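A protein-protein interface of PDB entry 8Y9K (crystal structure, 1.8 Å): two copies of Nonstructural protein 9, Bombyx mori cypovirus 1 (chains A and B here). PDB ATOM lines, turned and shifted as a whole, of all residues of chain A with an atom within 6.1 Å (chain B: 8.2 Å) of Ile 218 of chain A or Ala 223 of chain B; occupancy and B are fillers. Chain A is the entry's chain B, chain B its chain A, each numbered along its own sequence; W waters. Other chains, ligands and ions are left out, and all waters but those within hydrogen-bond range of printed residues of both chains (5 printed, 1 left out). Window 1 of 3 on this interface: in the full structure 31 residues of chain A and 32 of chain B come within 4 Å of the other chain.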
ATOM      1  N   GLN A 207     -17.769 -15.715 -22.230  1.00  0.00           N
ATOM      2  CA  GLN A 207     -17.841 -14.295 -21.901  1.00  0.00           C
ATOM      3  C   GLN A 207     -16.533 -13.768 -21.337  1.00  0.00           C
ATOM      4  O   GLN A 207     -16.230 -12.576 -21.491  1.00  0.00           O
ATOM      5  CB  GLN A 207     -18.978 -14.016 -20.908  1.00  0.00           C
ATOM      6  CG  GLN A 207     -18.849 -14.719 -19.564  1.00  0.00           C
ATOM      7  CD  GLN A 207     -19.855 -14.233 -18.516  1.00  0.00           C
ATOM      8  OE1 GLN A 207     -20.508 -13.200 -18.684  1.00  0.00           O
ATOM      9  NE2 GLN A 207     -20.003 -15.009 -17.435  1.00  0.00           N
ATOM     10  N   ILE A 214     -14.693  -8.759 -15.487  1.00  0.00           N
ATOM     11  CA  ILE A 214     -16.054  -8.782 -14.995  1.00  0.00           C
ATOM     12  C   ILE A 214     -16.012  -8.752 -13.483  1.00  0.00           C
ATOM     13  O   ILE A 214     -15.282  -9.540 -12.871  1.00  0.00           O
ATOM     14  CB  ILE A 214     -16.791 -10.030 -15.514  1.00  0.00           C
ATOM     15  CG1 ILE A 214     -16.638 -10.132 -17.041  1.00  0.00           C
ATOM     16  CG2 ILE A 214     -18.262  -9.953 -15.178  1.00  0.00           C
ATOM     17  CD1 ILE A 214     -17.057 -11.474 -17.631  1.00  0.00           C
ATOM     18  N   SER A 215     -16.787  -7.869 -12.886  1.00  0.00           N
ATOM     19  CA  SER A 215     -16.792  -7.790 -11.441  1.00  0.00           C
ATOM     20  C   SER A 215     -17.467  -9.027 -10.858  1.00  0.00           C
ATOM     21  O   SER A 215     -18.267  -9.698 -11.516  1.00  0.00           O
ATOM     22  CB  SER A 215     -17.547  -6.551 -10.974  1.00  0.00           C
ATOM     23  OG  SER A 215     -18.838  -6.511 -11.552  1.00  0.00           O
ATOM     24  N   ALA A 216     -17.138  -9.326  -9.601  1.00  0.00           N
ATOM     25  CA  ALA A 216     -17.642 -10.547  -8.982  1.00  0.00           C
ATOM     26  C   ALA A 216     -19.169 -10.552  -8.908  1.00  0.00           C
ATOM     27  O   ALA A 216     -19.790 -11.609  -9.068  1.00  0.00           O
ATOM     28  CB  ALA A 216     -17.036 -10.735  -7.590  1.00  0.00           C
ATOM     29  N   ASP A 217     -19.795  -9.396  -8.662  1.00  0.00           N
ATOM     30  CA  ASP A 217     -21.250  -9.410  -8.510  1.00  0.00           C
ATOM     31  C   ASP A 217     -21.917  -9.745  -9.851  1.00  0.00           C
ATOM     32  O   ASP A 217     -22.937 -10.448  -9.896  1.00  0.00           O
ATOM     33  CB  ASP A 217     -21.777  -8.090  -7.904  1.00  0.00           C
ATOM     34  CG  ASP A 217     -21.409  -6.820  -8.688  1.00  0.00           C
ATOM     35  OD1 ASP A 217     -20.534  -6.840  -9.576  1.00  0.00           O
ATOM     36  OD2 ASP A 217     -22.046  -5.778  -8.394  1.00  0.00           O
ATOM     37  N   ILE A 218     -21.330  -9.291 -10.960  1.00  0.00           N
ATOM     38  CA  ILE A 218     -21.857  -9.652 -12.272  1.00  0.00           C
ATOM     39  C   ILE A 218     -21.560 -11.115 -12.585  1.00  0.00           C
ATOM     40  O   ILE A 218     -22.411 -11.826 -13.135  1.00  0.00           O
ATOM     41  CB  ILE A 218     -21.278  -8.702 -13.337  1.00  0.00           C
ATOM     42  CG1 ILE A 218     -21.618  -7.237 -13.018  1.00  0.00           C
ATOM     43  CG2 ILE A 218     -21.756  -9.076 -14.719  1.00  0.00           C
ATOM     44  CD1 ILE A 218     -23.113  -6.936 -12.868  1.00  0.00           C
ATOM     45  N   ILE A 219     -20.361 -11.598 -12.243  1.00  0.00           N
ATOM     46  CA  ILE A 219     -20.072 -13.016 -12.448  1.00  0.00           C
ATOM     47  C   ILE A 219     -21.110 -13.867 -11.735  1.00  0.00           C
ATOM     48  O   ILE A 219     -21.697 -14.795 -12.308  1.00  0.00           O
ATOM     49  CB  ILE A 219     -18.652 -13.359 -11.963  1.00  0.00           C
ATOM     50  CG1 ILE A 219     -17.613 -12.753 -12.905  1.00  0.00           C
ATOM     51  CG2 ILE A 219     -18.476 -14.879 -11.874  1.00  0.00           C
ATOM     52  CD1 ILE A 219     -16.199 -12.831 -12.397  1.00  0.00           C
ATOM     53  N   CYS A 220     -21.373 -13.544 -10.472  1.00  0.00           N
ATOM     54  CA  CYS A 220     -22.204 -14.412  -9.651  1.00  0.00           C
ATOM     55  C   CYS A 220     -23.671 -14.346 -10.061  1.00  0.00           C
ATOM     56  O   CYS A 220     -24.358 -15.375 -10.068  1.00  0.00           O
ATOM     57  CB  CYS A 220     -22.020 -14.042  -8.178  1.00  0.00           C
ATOM     58  SG  CYS A 220     -20.425 -14.588  -7.538  1.00  0.00           S
ATOM     59  N   GLU A 221     -24.178 -13.157 -10.380  1.00  0.00           N
ATOM     60  CA  GLU A 221     -25.610 -12.985 -10.574  1.00  0.00           C
ATOM     61  C   GLU A 221     -26.023 -12.380 -11.912  1.00  0.00           C
ATOM     62  O   GLU A 221     -27.221 -12.398 -12.224  1.00  0.00           O
ATOM     63  CB  GLU A 221     -26.172 -12.116  -9.427  1.00  0.00           C
ATOM     64  CG  GLU A 221     -25.895 -12.740  -8.051  1.00  0.00           C
ATOM     65  CD  GLU A 221     -26.647 -12.088  -6.901  1.00  0.00           C
ATOM     66  OE1 GLU A 221     -26.155 -11.073  -6.366  1.00  0.00           O
ATOM     67  OE2 GLU A 221     -27.703 -12.625  -6.510  1.00  0.00           O
ATOM     68  N   GLY A 222     -25.091 -11.874 -12.711  1.00  0.00           N
ATOM     69  CA  GLY A 222     -25.394 -11.272 -13.989  1.00  0.00           C
ATOM     70  C   GLY A 222     -24.587 -11.937 -15.097  1.00  0.00           C
ATOM     71  O   GLY A 222     -24.266 -13.121 -15.036  1.00  0.00           O
ATOM     72  N   ALA A 223     -24.266 -11.155 -16.125  1.00  0.00           N
ATOM     73  CA  ALA A 223     -23.500 -11.675 -17.252  1.00  0.00           C
ATOM     74  C   ALA A 223     -23.000 -10.528 -18.118  1.00  0.00           C
ATOM     75  O   ALA A 223     -23.538  -9.417 -18.082  1.00  0.00           O
ATOM     76  CB  ALA A 223     -24.334 -12.653 -18.094  1.00  0.00           C
ATOM     77  N   ALA A 224     -21.957 -10.814 -18.903  1.00  0.00           N
ATOM     78  CA  ALA A 224     -21.491  -9.875 -19.914  1.00  0.00           C
ATOM     79  C   ALA A 224     -22.231 -10.042 -21.241  1.00  0.00           C
ATOM     80  O   ALA A 224     -21.774  -9.511 -22.255  1.00  0.00           O
ATOM     81  CB  ALA A 224     -19.979 -10.033 -20.131  1.00  0.00           C
ATOM     82  N   TYR A 225     -23.351 -10.772 -21.248  1.00  0.00           N
ATOM     83  CA  TYR A 225     -24.198 -10.993 -22.418  1.00  0.00           C
ATOM     84  C   TYR A 225     -25.644 -10.905 -21.934  1.00  0.00           C
ATOM     85  O   TYR A 225     -25.910 -10.886 -20.729  1.00  0.00           O
ATOM     86  CB  TYR A 225     -23.939 -12.347 -23.083  1.00  0.00           C
ATOM     87  CG  TYR A 225     -24.056 -13.454 -22.090  1.00  0.00           C
ATOM     88  CD1 TYR A 225     -25.274 -14.043 -21.798  1.00  0.00           C
ATOM     89  CD2 TYR A 225     -22.939 -13.893 -21.407  1.00  0.00           C
ATOM     90  CE1 TYR A 225     -25.373 -15.059 -20.860  1.00  0.00           C
ATOM     91  CE2 TYR A 225     -23.026 -14.893 -20.473  1.00  0.00           C
ATOM     92  CZ  TYR A 225     -24.236 -15.473 -20.197  1.00  0.00           C
ATOM     93  OH  TYR A 225     -24.286 -16.464 -19.249  1.00  0.00           O
ATOM     94  N   ARG A 226     -26.582 -10.869 -22.879  1.00  0.00           N
ATOM     95  CA  ARG A 226     -28.011 -10.918 -22.575  1.00  0.00           C
ATOM     96  C   ARG A 226     -28.649 -12.073 -23.350  1.00  0.00           C
ATOM     97  O   ARG A 226     -27.984 -12.818 -24.077  1.00  0.00           O
ATOM     98  CB  ARG A 226     -28.696  -9.586 -22.909  1.00  0.00           C
ATOM     99  CG  ARG A 226     -28.205  -8.421 -22.055  1.00  0.00           C
ATOM    100  CD  ARG A 226     -29.117  -7.205 -22.029  1.00  0.00           C
ATOM    101  NE  ARG A 226     -28.989  -6.339 -23.198  1.00  0.00           N
ATOM    102  CZ  ARG A 226     -28.155  -5.313 -23.284  1.00  0.00           C
ATOM    103  NH1 ARG A 226     -27.301  -5.035 -22.312  1.00  0.00           N
ATOM    104  NH2 ARG A 226     -28.155  -4.564 -24.384  1.00  0.00           N
ATOM    105  N   LYS B 159     -27.007  -4.733 -30.073  1.00  0.00           N
ATOM    106  CA  LYS B 159     -27.585  -6.060 -30.254  1.00  0.00           C
ATOM    107  C   LYS B 159     -28.279  -6.239 -31.595  1.00  0.00           C
ATOM    108  O   LYS B 159     -28.979  -7.240 -31.782  1.00  0.00           O
ATOM    109  CB  LYS B 159     -28.594  -6.355 -29.144  1.00  0.00           C
ATOM    110  CG  LYS B 159     -28.047  -6.285 -27.744  1.00  0.00           C
ATOM    111  CD  LYS B 159     -26.973  -7.318 -27.522  1.00  0.00           C
ATOM    112  CE  LYS B 159     -26.461  -7.274 -26.088  1.00  0.00           C
ATOM    113  NZ  LYS B 159     -25.253  -8.107 -25.890  1.00  0.00           N
ATOM    114  N   ILE B 203     -37.164  -4.782 -16.036  1.00  0.00           N
ATOM    115  CA  ILE B 203     -35.998  -5.303 -15.321  1.00  0.00           C
ATOM    116  C   ILE B 203     -34.735  -4.574 -15.760  1.00  0.00           C
ATOM    117  O   ILE B 203     -33.783  -4.442 -14.978  1.00  0.00           O
ATOM    118  CB  ILE B 203     -35.896  -6.843 -15.524  1.00  0.00           C
ATOM    119  CG1 ILE B 203     -34.927  -7.479 -14.529  1.00  0.00           C
ATOM    120  CG2 ILE B 203     -35.472  -7.177 -16.945  1.00  0.00           C
ATOM    121  CD1 ILE B 203     -34.902  -9.005 -14.577  1.00  0.00           C
ATOM    122  N   GLN B 204     -34.688  -4.106 -17.013  1.00  0.00           N
ATOM    123  CA  GLN B 204     -33.510  -3.372 -17.481  1.00  0.00           C
ATOM    124  C   GLN B 204     -33.281  -2.089 -16.692  1.00  0.00           C
ATOM    125  O   GLN B 204     -32.169  -1.552 -16.724  1.00  0.00           O
ATOM    126  CB  GLN B 204     -33.660  -3.043 -18.964  1.00  0.00           C
ATOM    127  CG  GLN B 204     -33.650  -4.261 -19.868  1.00  0.00           C
ATOM    128  CD  GLN B 204     -35.034  -4.727 -20.215  1.00  0.00           C
ATOM    129  OE1 GLN B 204     -35.954  -4.631 -19.395  1.00  0.00           O
ATOM    130  NE2 GLN B 204     -35.203  -5.225 -21.435  1.00  0.00           N
ATOM    131  N   GLN B 207     -32.585  -3.295 -12.408  1.00  0.00           N
ATOM    132  CA  GLN B 207     -31.262  -3.794 -12.023  1.00  0.00           C
ATOM    133  C   GLN B 207     -30.399  -2.720 -11.374  1.00  0.00           C
ATOM    134  O   GLN B 207     -29.544  -3.037 -10.543  1.00  0.00           O
ATOM    135  CB  GLN B 207     -30.549  -4.397 -13.249  1.00  0.00           C
ATOM    136  CG  GLN B 207     -30.324  -3.406 -14.384  1.00  0.00           C
ATOM    137  CD  GLN B 207     -29.412  -3.926 -15.476  1.00  0.00           C
ATOM    138  OE1 GLN B 207     -28.728  -4.935 -15.307  1.00  0.00           O
ATOM    139  NE2 GLN B 207     -29.442  -3.261 -16.628  1.00  0.00           N
ATOM    140  N   THR B 211     -28.023  -3.248  -7.412  1.00  0.00           N
ATOM    141  CA  THR B 211     -26.585  -3.326  -7.600  1.00  0.00           C
ATOM    142  C   THR B 211     -26.000  -1.971  -7.216  1.00  0.00           C
ATOM    143  O   THR B 211     -26.567  -0.932  -7.600  1.00  0.00           O
ATOM    144  CB  THR B 211     -26.258  -3.627  -9.056  1.00  0.00           C
ATOM    145  OG1 THR B 211     -26.641  -2.486  -9.841  1.00  0.00           O
ATOM    146  CG2 THR B 211     -27.068  -4.819  -9.531  1.00  0.00           C
ATOM    147  N   PRO B 212     -24.926  -1.915  -6.426  1.00  0.00           N
ATOM    148  CA  PRO B 212     -24.351  -0.593  -6.117  1.00  0.00           C
ATOM    149  C   PRO B 212     -24.021   0.204  -7.381  1.00  0.00           C
ATOM    150  O   PRO B 212     -24.285   1.410  -7.455  1.00  0.00           O
ATOM    151  CB  PRO B 212     -23.099  -0.921  -5.290  1.00  0.00           C
ATOM    152  CG  PRO B 212     -22.858  -2.377  -5.413  1.00  0.00           C
ATOM    153  CD  PRO B 212     -24.081  -3.039  -5.973  1.00  0.00           C
ATOM    154  N   PHE B 213     -23.389  -0.435  -8.361  1.00  0.00           N
ATOM    155  CA  PHE B 213     -23.117   0.193  -9.645  1.00  0.00           C
ATOM    156  C   PHE B 213     -22.834  -0.915 -10.653  1.00  0.00           C
ATOM    157  O   PHE B 213     -22.460  -2.029 -10.283  1.00  0.00           O
ATOM    158  CB  PHE B 213     -21.950   1.175  -9.574  1.00  0.00           C
ATOM    159  CG  PHE B 213     -20.617   0.541  -9.768  1.00  0.00           C
ATOM    160  CD1 PHE B 213     -20.042  -0.222  -8.773  1.00  0.00           C
ATOM    161  CD2 PHE B 213     -19.950   0.691 -10.962  1.00  0.00           C
ATOM    162  CE1 PHE B 213     -18.825  -0.809  -8.960  1.00  0.00           C
ATOM    163  CE2 PHE B 213     -18.719   0.113 -11.153  1.00  0.00           C
ATOM    164  CZ  PHE B 213     -18.160  -0.639 -10.153  1.00  0.00           C
ATOM    165  N   ILE B 214     -23.073  -0.608 -11.925  1.00  0.00           N
ATOM    166  CA  ILE B 214     -22.836  -1.512 -13.039  1.00  0.00           C
ATOM    167  C   ILE B 214     -21.881  -0.812 -14.000  1.00  0.00           C
ATOM    168  O   ILE B 214     -22.101   0.352 -14.351  1.00  0.00           O
ATOM    169  CB  ILE B 214     -24.159  -1.868 -13.747  1.00  0.00           C
ATOM    170  CG1 ILE B 214     -25.205  -2.348 -12.734  1.00  0.00           C
ATOM    171  CG2 ILE B 214     -23.923  -2.934 -14.810  1.00  0.00           C
ATOM    172  CD1 ILE B 214     -26.607  -2.430 -13.281  1.00  0.00           C
ATOM    173  N   SER B 215     -20.824  -1.500 -14.412  1.00  0.00           N
ATOM    174  CA  SER B 215     -19.869  -0.884 -15.318  1.00  0.00           C
ATOM    175  C   SER B 215     -20.501  -0.699 -16.692  1.00  0.00           C
ATOM    176  O   SER B 215     -21.462  -1.373 -17.058  1.00  0.00           O
ATOM    177  CB  SER B 215     -18.599  -1.734 -15.420  1.00  0.00           C
ATOM    178  OG  SER B 215     -18.858  -3.062 -15.839  1.00  0.00           O
ATOM    179  N   ASP B 217     -19.568  -1.414 -19.728  1.00  0.00           N
ATOM    180  CA  ASP B 217     -19.571  -2.508 -20.695  1.00  0.00           C
ATOM    181  C   ASP B 217     -20.690  -3.494 -20.378  1.00  0.00           C
ATOM    182  O   ASP B 217     -21.318  -4.028 -21.297  1.00  0.00           O
ATOM    183  CB  ASP B 217     -18.187  -3.168 -20.770  1.00  0.00           C
ATOM    184  CG  ASP B 217     -17.667  -3.691 -19.434  1.00  0.00           C
ATOM    185  OD1 ASP B 217     -18.273  -3.441 -18.371  1.00  0.00           O
ATOM    186  OD2 ASP B 217     -16.640  -4.406 -19.470  1.00  0.00           O
ATOM    187  N   ILE B 218     -20.986  -3.698 -19.090  1.00  0.00           N
ATOM    188  CA  ILE B 218     -22.101  -4.562 -18.703  1.00  0.00           C
ATOM    189  C   ILE B 218     -23.433  -3.891 -18.987  1.00  0.00           C
ATOM    190  O   ILE B 218     -24.388  -4.539 -19.442  1.00  0.00           O
ATOM    191  CB  ILE B 218     -21.970  -4.956 -17.217  1.00  0.00           C
ATOM    192  CG1 ILE B 218     -20.621  -5.662 -16.988  1.00  0.00           C
ATOM    193  CG2 ILE B 218     -23.169  -5.761 -16.749  1.00  0.00           C
ATOM    194  CD1 ILE B 218     -20.379  -6.864 -17.858  1.00  0.00           C
ATOM    195  N   ILE B 219     -23.536  -2.588 -18.710  1.00  0.00           N
ATOM    196  CA  ILE B 219     -24.772  -1.876 -19.045  1.00  0.00           C
ATOM    197  C   ILE B 219     -25.081  -2.031 -20.527  1.00  0.00           C
ATOM    198  O   ILE B 219     -26.203  -2.368 -20.919  1.00  0.00           O
ATOM    199  CB  ILE B 219     -24.674  -0.389 -18.657  1.00  0.00           C
ATOM    200  CG1 ILE B 219     -24.723  -0.222 -17.135  1.00  0.00           C
ATOM    201  CG2 ILE B 219     -25.800   0.411 -19.314  1.00  0.00           C
ATOM    202  CD1 ILE B 219     -24.353   1.171 -16.649  1.00  0.00           C
ATOM    203  N   CYS B 220     -24.077  -1.800 -21.370  1.00  0.00           N
ATOM    204  CA  CYS B 220     -24.306  -1.721 -22.810  1.00  0.00           C
ATOM    205  C   CYS B 220     -24.600  -3.094 -23.414  1.00  0.00           C
ATOM    206  O   CYS B 220     -25.470  -3.219 -24.283  1.00  0.00           O
ATOM    207  CB  CYS B 220     -23.104  -1.070 -23.487  1.00  0.00           C
ATOM    208  SG  CYS B 220     -22.987   0.720 -23.205  1.00  0.00           S
ATOM    209  N   GLU B 221     -23.890  -4.136 -22.977  1.00  0.00           N
ATOM    210  CA  GLU B 221     -23.962  -5.436 -23.643  1.00  0.00           C
ATOM    211  C   GLU B 221     -24.318  -6.608 -22.736  1.00  0.00           C
ATOM    212  O   GLU B 221     -24.628  -7.685 -23.255  1.00  0.00           O
ATOM    213  CB  GLU B 221     -22.616  -5.722 -24.339  1.00  0.00           C
ATOM    214  CG  GLU B 221     -22.231  -4.654 -25.351  1.00  0.00           C
ATOM    215  CD  GLU B 221     -21.056  -5.031 -26.235  1.00  0.00           C
ATOM    216  OE1 GLU B 221     -19.908  -4.814 -25.798  1.00  0.00           O
ATOM    217  OE2 GLU B 221     -21.291  -5.542 -27.346  1.00  0.00           O
ATOM    218  N   GLY B 222     -24.338  -6.427 -21.422  1.00  0.00           N
ATOM    219  CA  GLY B 222     -24.651  -7.483 -20.488  1.00  0.00           C
ATOM    220  C   GLY B 222     -25.793  -7.061 -19.581  1.00  0.00           C
ATOM    221  O   GLY B 222     -26.669  -6.286 -19.968  1.00  0.00           O
ATOM    222  N   ALA B 223     -25.770  -7.576 -18.357  1.00  0.00           N
ATOM    223  CA  ALA B 223     -26.816  -7.251 -17.393  1.00  0.00           C
ATOM    224  C   ALA B 223     -26.370  -7.697 -16.010  1.00  0.00           C
ATOM    225  O   ALA B 223     -25.482  -8.541 -15.870  1.00  0.00           O
ATOM    226  CB  ALA B 223     -28.151  -7.914 -17.767  1.00  0.00           C
ATOM    227  N   ALA B 224     -26.988  -7.108 -14.986  1.00  0.00           N
ATOM    228  CA  ALA B 224     -26.795  -7.563 -13.617  1.00  0.00           C
ATOM    229  C   ALA B 224     -27.752  -8.698 -13.255  1.00  0.00           C
ATOM    230  O   ALA B 224     -27.854  -9.053 -12.079  1.00  0.00           O
ATOM    231  CB  ALA B 224     -26.971  -6.399 -12.635  1.00  0.00           C
ATOM    232  N   TYR B 225     -28.403  -9.308 -14.246  1.00  0.00           N
ATOM    233  CA  TYR B 225     -29.326 -10.428 -14.062  1.00  0.00           C
ATOM    234  C   TYR B 225     -29.071 -11.406 -15.201  1.00  0.00           C
ATOM    235  O   TYR B 225     -28.335 -11.098 -16.147  1.00  0.00           O
ATOM    236  CB  TYR B 225     -30.790  -9.977 -14.056  1.00  0.00           C
ATOM    237  CG  TYR B 225     -31.122  -9.193 -15.289  1.00  0.00           C
ATOM    238  CD1 TYR B 225     -31.528  -9.837 -16.453  1.00  0.00           C
ATOM    239  CD2 TYR B 225     -31.019  -7.817 -15.304  1.00  0.00           C
ATOM    240  CE1 TYR B 225     -31.830  -9.119 -17.596  1.00  0.00           C
ATOM    241  CE2 TYR B 225     -31.310  -7.090 -16.444  1.00  0.00           C
ATOM    242  CZ  TYR B 225     -31.706  -7.750 -17.580  1.00  0.00           C
ATOM    243  OH  TYR B 225     -31.994  -7.021 -18.705  1.00  0.00           O
ATOM    244  N   ARG B 226     -29.676 -12.586 -15.114  1.00  0.00           N
ATOM    245  CA  ARG B 226     -29.614 -13.572 -16.194  1.00  0.00           C
ATOM    246  C   ARG B 226     -31.031 -13.957 -16.597  1.00  0.00           C
ATOM    247  O   ARG B 226     -32.012 -13.449 -16.052  1.00  0.00           O
ATOM    248  CB  ARG B 226     -28.803 -14.805 -15.772  1.00  0.00           C
ATOM    249  CG  ARG B 226     -27.324 -14.475 -15.491  1.00  0.00           C
ATOM    250  CD  ARG B 226     -26.388 -15.670 -15.507  1.00  0.00           C
ATOM    251  NE  ARG B 226     -26.401 -16.455 -14.281  1.00  0.00           N
ATOM    252  CZ  ARG B 226     -25.593 -16.249 -13.252  1.00  0.00           C
ATOM    253  NH1 ARG B 226     -24.735 -15.239 -13.235  1.00  0.00           N
ATOM    254  NH2 ARG B 226     -25.639 -17.080 -12.217  1.00  0.00           N
ATOM    255  N   SER B 227     -31.135 -14.877 -17.553  1.00  0.00           N
ATOM    256  CA  SER B 227     -32.411 -15.078 -18.239  1.00  0.00           C
ATOM    257  C   SER B 227     -33.531 -15.505 -17.296  1.00  0.00           C
ATOM    258  O   SER B 227     -34.658 -15.005 -17.411  1.00  0.00           O
ATOM    259  CB  SER B 227     -32.245 -16.096 -19.365  1.00  0.00           C
ATOM    260  OG  SER B 227     -31.287 -15.654 -20.311  1.00  0.00           O
ATOM    261  N   ASP B 229     -34.041 -14.646 -14.376  1.00  0.00           N
ATOM    262  CA  ASP B 229     -34.503 -13.502 -13.604  1.00  0.00           C
ATOM    263  C   ASP B 229     -35.597 -12.729 -14.329  1.00  0.00           C
ATOM    264  O   ASP B 229     -36.440 -12.097 -13.684  1.00  0.00           O
ATOM    265  CB  ASP B 229     -33.326 -12.575 -13.297  1.00  0.00           C
ATOM    266  CG  ASP B 229     -32.304 -13.234 -12.429  1.00  0.00           C
ATOM    267  OD1 ASP B 229     -32.693 -13.830 -11.410  1.00  0.00           O
ATOM    268  OD2 ASP B 229     -31.110 -13.174 -12.768  1.00  0.00           O
ATOM    269  N   VAL B 230     -35.591 -12.754 -15.660  1.00  0.00           N
ATOM    270  CA  VAL B 230     -36.616 -12.045 -16.421  1.00  0.00           C
ATOM    271  C   VAL B 230     -38.004 -12.604 -16.113  1.00  0.00           C
ATOM    272  O   VAL B 230     -38.957 -11.850 -15.877  1.00  0.00           O
ATOM    273  CB  VAL B 230     -36.307 -12.108 -17.927  1.00  0.00           C
ATOM    274  CG1 VAL B 230     -37.402 -11.390 -18.715  1.00  0.00           C
ATOM    275  CG2 VAL B 230     -34.940 -11.489 -18.218  1.00  0.00           C
ATOM    276  N   PHE B 269     -32.060  -9.947  -6.953  1.00  0.00           N
ATOM    277  CA  PHE B 269     -32.513 -10.996  -7.854  1.00  0.00           C
ATOM    278  C   PHE B 269     -32.429 -12.378  -7.231  1.00  0.00           C
ATOM    279  O   PHE B 269     -33.152 -13.281  -7.670  1.00  0.00           O
ATOM    280  CB  PHE B 269     -31.719 -10.947  -9.157  1.00  0.00           C
ATOM    281  CG  PHE B 269     -32.010  -9.733  -9.972  1.00  0.00           C
ATOM    282  CD1 PHE B 269     -33.300  -9.444 -10.362  1.00  0.00           C
ATOM    283  CD2 PHE B 269     -30.996  -8.869 -10.353  1.00  0.00           C
ATOM    284  CE1 PHE B 269     -33.595  -8.318 -11.096  1.00  0.00           C
ATOM    285  CE2 PHE B 269     -31.280  -7.751 -11.107  1.00  0.00           C
ATOM    286  CZ  PHE B 269     -32.582  -7.466 -11.473  1.00  0.00           C
HETATM  287  O   HOH W   1     -20.081  -4.077 -13.233  1.00  0.00           O
HETATM  288  O   HOH W   2     -20.974  -4.410 -10.781  1.00  0.00           O
HETATM  289  O   HOH W   3     -25.520  -8.850 -10.372  1.00  0.00           O
HETATM  290  O   HOH W   4     -18.214  -5.917 -14.435  1.00  0.00           O
HETATM  291  O   HOH W   5     -28.020 -11.455 -18.919  1.00  0.00           O
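The backbone carbonyl oxygen (O) of Cys 220 of chain B sits at hydrogen-bond distance from the guanidinium group (NH2) of Arg 226 of chain A (3.0 Å).
The guanidinium group of Arg 226 of chain B is in hydrogen-bond range of the backbone carbonyl oxygen of Gly 222 of chain A (2.8 Å).
N of Ala 223 of chain A is in hydrogen-bond range of O of Ala 223 of chain B, 2.9 Å away.
The backbone carbonyl oxygen (O) of Ile 219 of chain B lies within hydrogen-bond range of the guanidinium group (NH1) of Arg 226 of chain A (3.2 Å).
The guanidinium group of Arg 226 of chain B lies within hydrogen-bond range of the backbone carbonyl oxygen of Cys 220 of chain A.
The backbone carbonyl oxygen (O) of Ile 219 of chain A sits at hydrogen-bond distance from the guanidinium group (NH1) of Arg 226 of chain B, at 3.2 Å.
NH1 of Arg 226 of chain A lies within hydrogen-bond range of O of Gly 222 of chain B.
The backbone carbonyl oxygen (O) of Glu 221 of chain A sits close to the backbone carbonyl oxygen (O) of Ala 224 of chain B (3.4 Å).
The backbone carbonyl oxygen of Ala 216 of chain A is in hydrogen-bond range of the side-chain sulfur of Cys 220 of chain A (3.4 Å).
O of Glu 221 of chain B sits at hydrogen-bond distance from NZ of Lys 159 of chain B (2.7 Å).
OD2 of Asp 229 of chain B lies within hydrogen-bond range of N of Arg 226 of chain B (2.8 Å).
The side-chain amide oxygen of Gln 207 of chain A lies within hydrogen-bond range of the backbone NH of Ala 224 of chain A, 2.8 Å away.
CA of Ala 224 of chain B touches CD1 of Ile 218 of chain A (3.8 Å).
Glu 221 of chain A touches Tyr 225 of chain B (O to CA, 3.4 Å).
Glu 221 of chain A touches Arg 226 of chain B.
CG2 of Ile 218 of chain B touches O of Ala 223 of chain A, 3.9 Å away.
Ala 223 of chain A touches Gly 222 of chain B.
Gly 222 of chain B touches Ala 224 of chain A (CA to C, 3.6 Å).
Tyr 225 of chain A touches Glu 221 of chain B (CA to O, 3.4 Å).
N of Tyr 225 of chain A touches CA of Gly 222 of chain B (3.6 Å).
NH1 of Arg 226 of chain A touches C of Glu 221 of chain B, 3.4 Å away.
Of chain B, only Ala 223 (3.9 Å) and Ala 224 (3.8 Å) come within 4 Å of Ile 218 of chain A.
Ala 223 of chain B touches just these residues of chain A: Ile 218, Gly 222 and Ala 223.
Gly 222 of chain A touches just these residues of chain B: Ala 223 (3.3 Å), Ala 224 (3.6 Å), Tyr 225 (3.6 Å) and Arg 226 (2.8 Å).
Of the printed residues of chain A, Arg 226 of chain B touches Ile 219, Cys 220, Glu 221 and Gly 222.
Of the printed residues of chain A, Ile 218 of chain B touches Ala 223 (3.9 Å) and Ala 224 (3.8 Å).
Of the 23 printed residues of chain B, 10 touch a printed residue of chain A.
Printed residues of chain B that touch a printed residue of chain A: Lys 159, Ile 218, Ile 219, Cys 220, Glu 221, Gly 222, Ala 223, Ala 224, Tyr 225 and Arg 226.
Hydrophobic or aromatic side chains of chain B that line the printed part of chain A: Ile 218 and Ala 224.
Of the 14 printed residues of chain A, 9 touch a printed residue of chain B.
Hydrophobic or aromatic side chains of chain A that line the printed part of chain B: Ile 218 and Ala 224.
Among the printed residues, no Asp or Glu carboxylate lies within 4 Å of a Lys or Arg side-chain nitrogen of the other chain.
Ile 218 of chain A touches Ala 224 of chain B, and with the chains exchanged Ala 224 of chain A touches Ile 218 of chain B.
Gly 222 of chain A touches Ala 224 of chain B, and with the chains exchanged Ala 224 of chain A touches Gly 222 of chain B.
Gly 222 of chain A touches Tyr 225 of chain B, and with the chains exchanged Tyr 225 of chain A touches Gly 222 of chain B.
Gly 222 of chain A touches Arg 226 of chain B, and with the chains exchanged Arg 226 of chain A touches Gly 222 of chain B.
Positions printed for both chains: 207, 214, 215, 217, 218, 219, 220, 221, 222, 223, 224, 225 and 226.
Water W2 lies within hydrogen-bond range of OD1 of Asp 217 of chain A (2.7 Å), O of Phe 213 of chain B (2.9 Å) and OG of Ser 215 of chain A (3.1 Å).
Water W5 lies within hydrogen-bond range of the backbone carbonyl oxygen of Tyr 225 of chain B and the backbone carbonyl oxygen of Tyr 225 of chain A.
Water W4 bridges the backbone NH (N) of Ser 215 of chain A and the side-chain hydroxyl (OG) of Ser 215 of chain B.
Water W3 lies within hydrogen-bond range of O of Ala 224 of chain B and O of Asp 217 of chain A.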
